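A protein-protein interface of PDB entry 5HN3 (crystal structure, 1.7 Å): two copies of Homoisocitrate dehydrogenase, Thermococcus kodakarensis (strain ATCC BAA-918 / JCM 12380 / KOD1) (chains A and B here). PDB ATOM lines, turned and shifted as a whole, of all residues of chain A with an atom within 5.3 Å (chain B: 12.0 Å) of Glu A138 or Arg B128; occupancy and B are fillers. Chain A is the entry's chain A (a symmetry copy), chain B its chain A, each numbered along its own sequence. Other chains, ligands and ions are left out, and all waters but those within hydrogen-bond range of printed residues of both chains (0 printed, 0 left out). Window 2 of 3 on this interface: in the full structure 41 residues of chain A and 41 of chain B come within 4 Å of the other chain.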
ATOM      1  N   PHE A 119      -8.364 -25.813 -25.233  1.00  0.00           N
ATOM      2  CA  PHE A 119      -7.358 -24.886 -25.706  1.00  0.00           C
ATOM      3  C   PHE A 119      -7.363 -23.636 -24.867  1.00  0.00           C
ATOM      4  O   PHE A 119      -8.206 -23.463 -23.986  1.00  0.00           O
ATOM      5  CB  PHE A 119      -7.590 -24.546 -27.185  1.00  0.00           C
ATOM      6  CG  PHE A 119      -8.850 -23.778 -27.453  1.00  0.00           C
ATOM      7  CD1 PHE A 119     -10.079 -24.434 -27.558  1.00  0.00           C
ATOM      8  CD2 PHE A 119      -8.814 -22.393 -27.659  1.00  0.00           C
ATOM      9  CE1 PHE A 119     -11.255 -23.721 -27.831  1.00  0.00           C
ATOM     10  CE2 PHE A 119      -9.990 -21.677 -27.938  1.00  0.00           C
ATOM     11  CZ  PHE A 119     -11.207 -22.343 -28.026  1.00  0.00           C
ATOM     12  N   ILE A 135     -13.213 -25.018 -23.869  1.00  0.00           N
ATOM     13  CA  ILE A 135     -13.733 -26.257 -24.346  1.00  0.00           C
ATOM     14  C   ILE A 135     -14.986 -25.972 -25.196  1.00  0.00           C
ATOM     15  O   ILE A 135     -15.771 -25.046 -24.885  1.00  0.00           O
ATOM     16  CB  ILE A 135     -14.060 -27.221 -23.156  1.00  0.00           C
ATOM     17  CG1 ILE A 135     -14.570 -28.552 -23.671  1.00  0.00           C
ATOM     18  CG2 ILE A 135     -15.102 -26.627 -22.233  1.00  0.00           C
ATOM     19  CD1 ILE A 135     -14.789 -29.594 -22.581  1.00  0.00           C
ATOM     20  N   THR A 136     -15.203 -26.758 -26.244  1.00  0.00           N
ATOM     21  CA  THR A 136     -16.439 -26.596 -27.019  1.00  0.00           C
ATOM     22  C   THR A 136     -17.310 -27.817 -27.012  1.00  0.00           C
ATOM     23  O   THR A 136     -16.856 -28.950 -26.773  1.00  0.00           O
ATOM     24  CB  THR A 136     -16.179 -26.221 -28.501  1.00  0.00           C
ATOM     25  OG1 THR A 136     -15.767 -27.384 -29.213  1.00  0.00           O
ATOM     26  CG2 THR A 136     -15.146 -25.154 -28.633  1.00  0.00           C
ATOM     27  N   ARG A 137     -18.582 -27.591 -27.316  1.00  0.00           N
ATOM     28  CA  ARG A 137     -19.509 -28.667 -27.465  1.00  0.00           C
ATOM     29  C   ARG A 137     -18.989 -29.712 -28.435  1.00  0.00           C
ATOM     30  O   ARG A 137     -19.122 -30.903 -28.174  1.00  0.00           O
ATOM     31  CB  ARG A 137     -20.878 -28.140 -27.927  1.00  0.00           C
ATOM     32  CG  ARG A 137     -21.859 -29.201 -28.379  1.00  0.00           C
ATOM     33  CD  ARG A 137     -23.269 -28.623 -28.473  1.00  0.00           C
ATOM     34  NE  ARG A 137     -23.534 -27.769 -27.314  1.00  0.00           N
ATOM     35  CZ  ARG A 137     -24.163 -28.157 -26.200  1.00  0.00           C
ATOM     36  NH1 ARG A 137     -24.317 -27.291 -25.211  1.00  0.00           N
ATOM     37  NH2 ARG A 137     -24.661 -29.390 -26.078  1.00  0.00           N
ATOM     38  N   GLU A 138     -18.444 -29.271 -29.571  1.00  0.00           N
ATOM     39  CA  GLU A 138     -18.026 -30.204 -30.621  1.00  0.00           C
ATOM     40  C   GLU A 138     -16.897 -31.137 -30.122  1.00  0.00           C
ATOM     41  O   GLU A 138     -16.942 -32.348 -30.330  1.00  0.00           O
ATOM     42  CB  GLU A 138     -17.666 -29.489 -31.954  1.00  0.00           C
ATOM     43  CG  GLU A 138     -16.861 -28.190 -31.868  1.00  0.00           C
ATOM     44  CD  GLU A 138     -17.675 -26.905 -31.536  1.00  0.00           C
ATOM     45  OE1 GLU A 138     -17.118 -25.791 -31.754  1.00  0.00           O
ATOM     46  OE2 GLU A 138     -18.839 -26.977 -31.041  1.00  0.00           O
ATOM     47  N   GLY A 139     -15.944 -30.568 -29.407  1.00  0.00           N
ATOM     48  CA  GLY A 139     -14.822 -31.347 -28.846  1.00  0.00           C
ATOM     49  C   GLY A 139     -15.293 -32.258 -27.724  1.00  0.00           C
ATOM     50  O   GLY A 139     -14.924 -33.460 -27.663  1.00  0.00           O
ATOM     51  N   ALA A 140     -16.164 -31.725 -26.863  1.00  0.00           N
ATOM     52  CA  ALA A 140     -16.753 -32.541 -25.793  1.00  0.00           C
ATOM     53  C   ALA A 140     -17.576 -33.710 -26.345  1.00  0.00           C
ATOM     54  O   ALA A 140     -17.443 -34.833 -25.877  1.00  0.00           O
ATOM     55  CB  ALA A 140     -17.578 -31.659 -24.838  1.00  0.00           C
ATOM     56  N   GLU A 141     -18.399 -33.490 -27.394  1.00  0.00           N
ATOM     57  CA  GLU A 141     -19.166 -34.563 -27.964  1.00  0.00           C
ATOM     58  C   GLU A 141     -18.314 -35.673 -28.550  1.00  0.00           C
ATOM     59  O   GLU A 141     -18.674 -36.848 -28.483  1.00  0.00           O
ATOM     60  CB  GLU A 141     -20.047 -34.048 -29.098  1.00  0.00           C
ATOM     61  CG  GLU A 141     -21.213 -33.216 -28.674  1.00  0.00           C
ATOM     62  CD  GLU A 141     -21.962 -32.739 -29.905  1.00  0.00           C
ATOM     63  OE1 GLU A 141     -21.901 -31.533 -30.206  1.00  0.00           O
ATOM     64  OE2 GLU A 141     -22.544 -33.607 -30.581  1.00  0.00           O
ATOM     65  N   ARG A 142     -17.222 -35.290 -29.175  1.00  0.00           N
ATOM     66  CA  ARG A 142     -16.372 -36.214 -29.893  1.00  0.00           C
ATOM     67  C   ARG A 142     -15.771 -37.224 -28.930  1.00  0.00           C
ATOM     68  O   ARG A 142     -15.806 -38.420 -29.158  1.00  0.00           O
ATOM     69  CB  ARG A 142     -15.248 -35.449 -30.575  1.00  0.00           C
ATOM     70  CG  ARG A 142     -14.285 -36.362 -31.313  1.00  0.00           C
ATOM     71  CD  ARG A 142     -13.311 -35.569 -32.145  1.00  0.00           C
ATOM     72  NE  ARG A 142     -12.392 -34.706 -31.388  1.00  0.00           N
ATOM     73  CZ  ARG A 142     -11.295 -34.148 -31.906  1.00  0.00           C
ATOM     74  NH1 ARG A 142     -10.535 -33.360 -31.187  1.00  0.00           N
ATOM     75  NH2 ARG A 142     -10.935 -34.367 -33.178  1.00  0.00           N
ATOM     76  N   PHE A 172     -19.519 -28.268 -17.882  1.00  0.00           N
ATOM     77  CA  PHE A 172     -19.940 -28.338 -19.276  1.00  0.00           C
ATOM     78  C   PHE A 172     -19.699 -29.706 -19.912  1.00  0.00           C
ATOM     79  O   PHE A 172     -20.564 -30.283 -20.543  1.00  0.00           O
ATOM     80  CB  PHE A 172     -19.181 -27.255 -20.038  1.00  0.00           C
ATOM     81  CG  PHE A 172     -19.540 -27.156 -21.493  1.00  0.00           C
ATOM     82  CD1 PHE A 172     -20.602 -26.349 -21.907  1.00  0.00           C
ATOM     83  CD2 PHE A 172     -18.811 -27.827 -22.453  1.00  0.00           C
ATOM     84  CE1 PHE A 172     -20.919 -26.246 -23.259  1.00  0.00           C
ATOM     85  CE2 PHE A 172     -19.116 -27.713 -23.804  1.00  0.00           C
ATOM     86  CZ  PHE A 172     -20.180 -26.930 -24.203  1.00  0.00           C
ATOM     87  N   ILE B 121     -12.838 -16.700 -13.165  1.00  0.00           N
ATOM     88  CA  ILE B 121     -14.225 -16.902 -13.509  1.00  0.00           C
ATOM     89  C   ILE B 121     -14.394 -18.151 -14.344  1.00  0.00           C
ATOM     90  O   ILE B 121     -13.478 -18.548 -15.054  1.00  0.00           O
ATOM     91  CB  ILE B 121     -14.712 -15.682 -14.326  1.00  0.00           C
ATOM     92  CG1 ILE B 121     -16.238 -15.684 -14.508  1.00  0.00           C
ATOM     93  CG2 ILE B 121     -14.030 -15.616 -15.679  1.00  0.00           C
ATOM     94  CD1 ILE B 121     -16.815 -14.275 -14.593  1.00  0.00           C
ATOM     95  N   GLY B 122     -15.579 -18.724 -14.307  1.00  0.00           N
ATOM     96  CA  GLY B 122     -15.941 -19.776 -15.207  1.00  0.00           C
ATOM     97  C   GLY B 122     -17.330 -19.544 -15.755  1.00  0.00           C
ATOM     98  O   GLY B 122     -18.220 -19.169 -15.021  1.00  0.00           O
ATOM     99  N   ALA B 123     -17.531 -19.832 -17.018  1.00  0.00           N
ATOM    100  CA  ALA B 123     -18.812 -19.515 -17.640  1.00  0.00           C
ATOM    101  C   ALA B 123     -19.073 -20.335 -18.876  1.00  0.00           C
ATOM    102  O   ALA B 123     -18.157 -20.831 -19.527  1.00  0.00           O
ATOM    103  CB  ALA B 123     -18.858 -18.014 -17.953  1.00  0.00           C
ATOM    104  N   VAL B 124     -20.349 -20.501 -19.192  1.00  0.00           N
ATOM    105  CA  VAL B 124     -20.740 -21.151 -20.431  1.00  0.00           C
ATOM    106  C   VAL B 124     -21.383 -20.061 -21.299  1.00  0.00           C
ATOM    107  O   VAL B 124     -21.844 -19.045 -20.773  1.00  0.00           O
ATOM    108  CB  VAL B 124     -21.690 -22.333 -20.203  1.00  0.00           C
ATOM    109  CG1 VAL B 124     -21.051 -23.345 -19.243  1.00  0.00           C
ATOM    110  CG2 VAL B 124     -23.015 -21.853 -19.646  1.00  0.00           C
ATOM    111  N   VAL B 125     -21.307 -20.233 -22.590  1.00  0.00           N
ATOM    112  CA  VAL B 125     -22.040 -19.365 -23.529  1.00  0.00           C
ATOM    113  C   VAL B 125     -22.313 -20.286 -24.681  1.00  0.00           C
ATOM    114  O   VAL B 125     -21.491 -20.421 -25.580  1.00  0.00           O
ATOM    115  CB  VAL B 125     -21.218 -18.129 -23.954  1.00  0.00           C
ATOM    116  CG1 VAL B 125     -19.929 -18.531 -24.649  1.00  0.00           C
ATOM    117  CG2 VAL B 125     -22.056 -17.209 -24.833  1.00  0.00           C
ATOM    118  N   ASN B 126     -23.456 -20.965 -24.606  1.00  0.00           N
ATOM    119  CA  ASN B 126     -23.530 -22.391 -25.037  1.00  0.00           C
ATOM    120  C   ASN B 126     -22.876 -22.770 -26.356  1.00  0.00           C
ATOM    121  O   ASN B 126     -22.806 -21.994 -27.307  1.00  0.00           O
ATOM    122  CB  ASN B 126     -24.947 -22.954 -24.926  1.00  0.00           C
ATOM    123  CG  ASN B 126     -25.132 -23.790 -23.664  1.00  0.00           C
ATOM    124  OD1 ASN B 126     -24.700 -24.942 -23.612  1.00  0.00           O
ATOM    125  ND2 ASN B 126     -25.769 -23.210 -22.639  1.00  0.00           N
ATOM    126  N   GLY B 127     -22.374 -23.988 -26.381  1.00  0.00           N
ATOM    127  CA  GLY B 127     -21.426 -24.397 -27.392  1.00  0.00           C
ATOM    128  C   GLY B 127     -19.987 -24.211 -26.952  1.00  0.00           C
ATOM    129  O   GLY B 127     -19.103 -24.811 -27.545  1.00  0.00           O
ATOM    130  N   ARG B 128     -19.741 -23.352 -25.952  1.00  0.00           N
ATOM    131  CA  ARG B 128     -18.396 -23.164 -25.397  1.00  0.00           C
ATOM    132  C   ARG B 128     -18.431 -22.862 -23.895  1.00  0.00           C
ATOM    133  O   ARG B 128     -19.367 -22.266 -23.385  1.00  0.00           O
ATOM    134  CB  ARG B 128     -17.623 -22.038 -26.112  1.00  0.00           C
ATOM    135  CG  ARG B 128     -17.760 -22.005 -27.642  1.00  0.00           C
ATOM    136  CD  ARG B 128     -17.236 -20.696 -28.272  1.00  0.00           C
ATOM    137  NE  ARG B 128     -15.841 -20.777 -28.738  1.00  0.00           N
ATOM    138  CZ  ARG B 128     -15.419 -21.522 -29.769  1.00  0.00           C
ATOM    139  NH1 ARG B 128     -14.138 -21.528 -30.106  1.00  0.00           N
ATOM    140  NH2 ARG B 128     -16.264 -22.286 -30.462  1.00  0.00           N
ATOM    141  N   ALA B 129     -17.401 -23.308 -23.179  1.00  0.00           N
ATOM    142  CA  ALA B 129     -17.194 -22.928 -21.803  1.00  0.00           C
ATOM    143  C   ALA B 129     -15.777 -22.442 -21.612  1.00  0.00           C
ATOM    144  O   ALA B 129     -14.846 -22.879 -22.301  1.00  0.00           O
ATOM    145  CB  ALA B 129     -17.509 -24.106 -20.861  1.00  0.00           C
ATOM    146  N   VAL B 130     -15.595 -21.560 -20.651  1.00  0.00           N
ATOM    147  CA  VAL B 130     -14.300 -21.001 -20.357  1.00  0.00           C
ATOM    148  C   VAL B 130     -14.069 -20.986 -18.880  1.00  0.00           C
ATOM    149  O   VAL B 130     -14.988 -20.829 -18.098  1.00  0.00           O
ATOM    150  CB  VAL B 130     -14.137 -19.572 -20.967  1.00  0.00           C
ATOM    151  CG1 VAL B 130     -15.218 -18.666 -20.436  1.00  0.00           C
ATOM    152  CG2 VAL B 130     -12.755 -18.998 -20.692  1.00  0.00           C
ATOM    153  N   ASP B 131     -12.812 -21.209 -18.494  1.00  0.00           N
ATOM    154  CA  ASP B 131     -12.325 -20.925 -17.165  1.00  0.00           C
ATOM    155  C   ASP B 131     -11.062 -20.093 -17.282  1.00  0.00           C
ATOM    156  O   ASP B 131     -10.173 -20.407 -18.077  1.00  0.00           O
ATOM    157  CB  ASP B 131     -11.993 -22.238 -16.392  1.00  0.00           C
ATOM    158  CG  ASP B 131     -13.214 -23.008 -16.014  1.00  0.00           C
ATOM    159  OD1 ASP B 131     -13.872 -22.670 -15.020  1.00  0.00           O
ATOM    160  OD2 ASP B 131     -13.555 -23.919 -16.752  1.00  0.00           O
ATOM    161  N   VAL B 132     -11.006 -19.034 -16.461  1.00  0.00           N
ATOM    162  CA  VAL B 132      -9.867 -18.187 -16.257  1.00  0.00           C
ATOM    163  C   VAL B 132      -9.431 -18.226 -14.818  1.00  0.00           C
ATOM    164  O   VAL B 132     -10.253 -18.046 -13.908  1.00  0.00           O
ATOM    165  CB  VAL B 132     -10.242 -16.691 -16.550  1.00  0.00           C
ATOM    166  CG1 VAL B 132      -9.040 -15.814 -16.300  1.00  0.00           C
ATOM    167  CG2 VAL B 132     -10.799 -16.583 -17.940  1.00  0.00           C
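Of chain B, only Arg B128 (3.8 Å) comes within 4 Å of Glu A138.
Of the printed residues of chain A, Arg B128 touches Phe A119 (3.7 Å), Ile A135 (3.3 Å), Thr A136 (3.6 Å) and Glu A138 (3.8 Å).
Of chain B, only Arg B128 and Ala B129 come within 4 Å of Ile A135.
Thr A136 touches just these residues of chain B: Gly B127 and Arg B128.
Arg A137 touches just these residues of chain B: Asn B126 (2.9 Å) and Gly B127 (2.8 Å).
No residue of chain B comes within 4 Å of Gly A139.
No residue of chain B comes within 4 Å of Ala A140.
No residue of chain B comes within 4 Å of Glu A141.
No residue of chain B comes within 4 Å of Arg A142.
Of the printed residues of chain A, Asn B126 touches Arg A137.
Printed residues of chain B within 4 Å of Phe A119: Arg B128 (3.7 Å).
Of the printed residues of chain A, Ala B129 touches Ile A135 and Phe A172.
Of the printed residues of chain B, Phe A172 touches Gly B127 (3.9 Å) and Ala B129 (3.7 Å).
Of the printed residues of chain A, Gly B127 touches Thr A136 (3.2 Å), Arg A137 (2.8 Å) and Phe A172 (3.9 Å).
Val B124 touches none of the printed residues of chain A.
Val B132 touches none of the printed residues of chain A.
No position is printed for both chains.
Of the 10 pairs that touch across the chains among the printed residues, none has its exchanged pair printed and touching as well.
Of the 12 printed residues of chain B, 4 touch a printed residue of chain A.
Printed residues of chain B that touch a printed residue of chain A: Asn B126, Gly B127, Arg B128 and Ala B129.
Hydrophobic or aromatic side chains of chain B within 4 Å of the printed part of chain A: Ala B129.
Of the 10 printed residues of chain A, 6 touch a printed residue of chain B.
Printed residues of chain A that touch a printed residue of chain B: Phe A119, Ile A135, Thr A136, Arg A137, Glu A138 and Phe A172.
Hydrophobic or aromatic side chains of chain A within 4 Å of the printed part of chain B: Phe A119, Ile A135 and Phe A172.
Among the printed residues, 10 pairs touch across the chains.
OG1 of Thr A136 sits close to OE1 of Glu A138, at 3.3 Å.
The side-chain hydroxyl (OG1) of Thr A136 sits at hydrogen-bond distance from the backbone NH (N) of Gly A139 (3.2 Å).
The guanidinium group (NH2) of Arg B128 lies within salt-bridge range of the side-chain carboxylate (OE1) of Glu A138 (3.8 Å).
The backbone carbonyl oxygen (O) of Ile A135 lies within hydrogen-bond range of the backbone NH (N) of Ala B129, at 2.9 Å.
The side-chain amide oxygen (OD1) of Asn B126 sits at hydrogen-bond distance from the guanidinium group (NH1) of Arg A137 (2.9 Å).
The backbone carbonyl oxygen of Gly B127 sits at hydrogen-bond distance from the backbone NH of Arg A137, at 2.8 Å.
Among the printed residues, pairs that only touch across the chains: Thr A136 with Gly B127 (3.2 Å), Ile A135 with Arg B128 (3.3 Å), Thr A136 with Arg B128 (3.6 Å), Phe A172 with Ala B129 (3.7 Å), Phe A119 with Arg B128 (3.7 Å) and Phe A172 with Gly B127 (3.9 Å).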
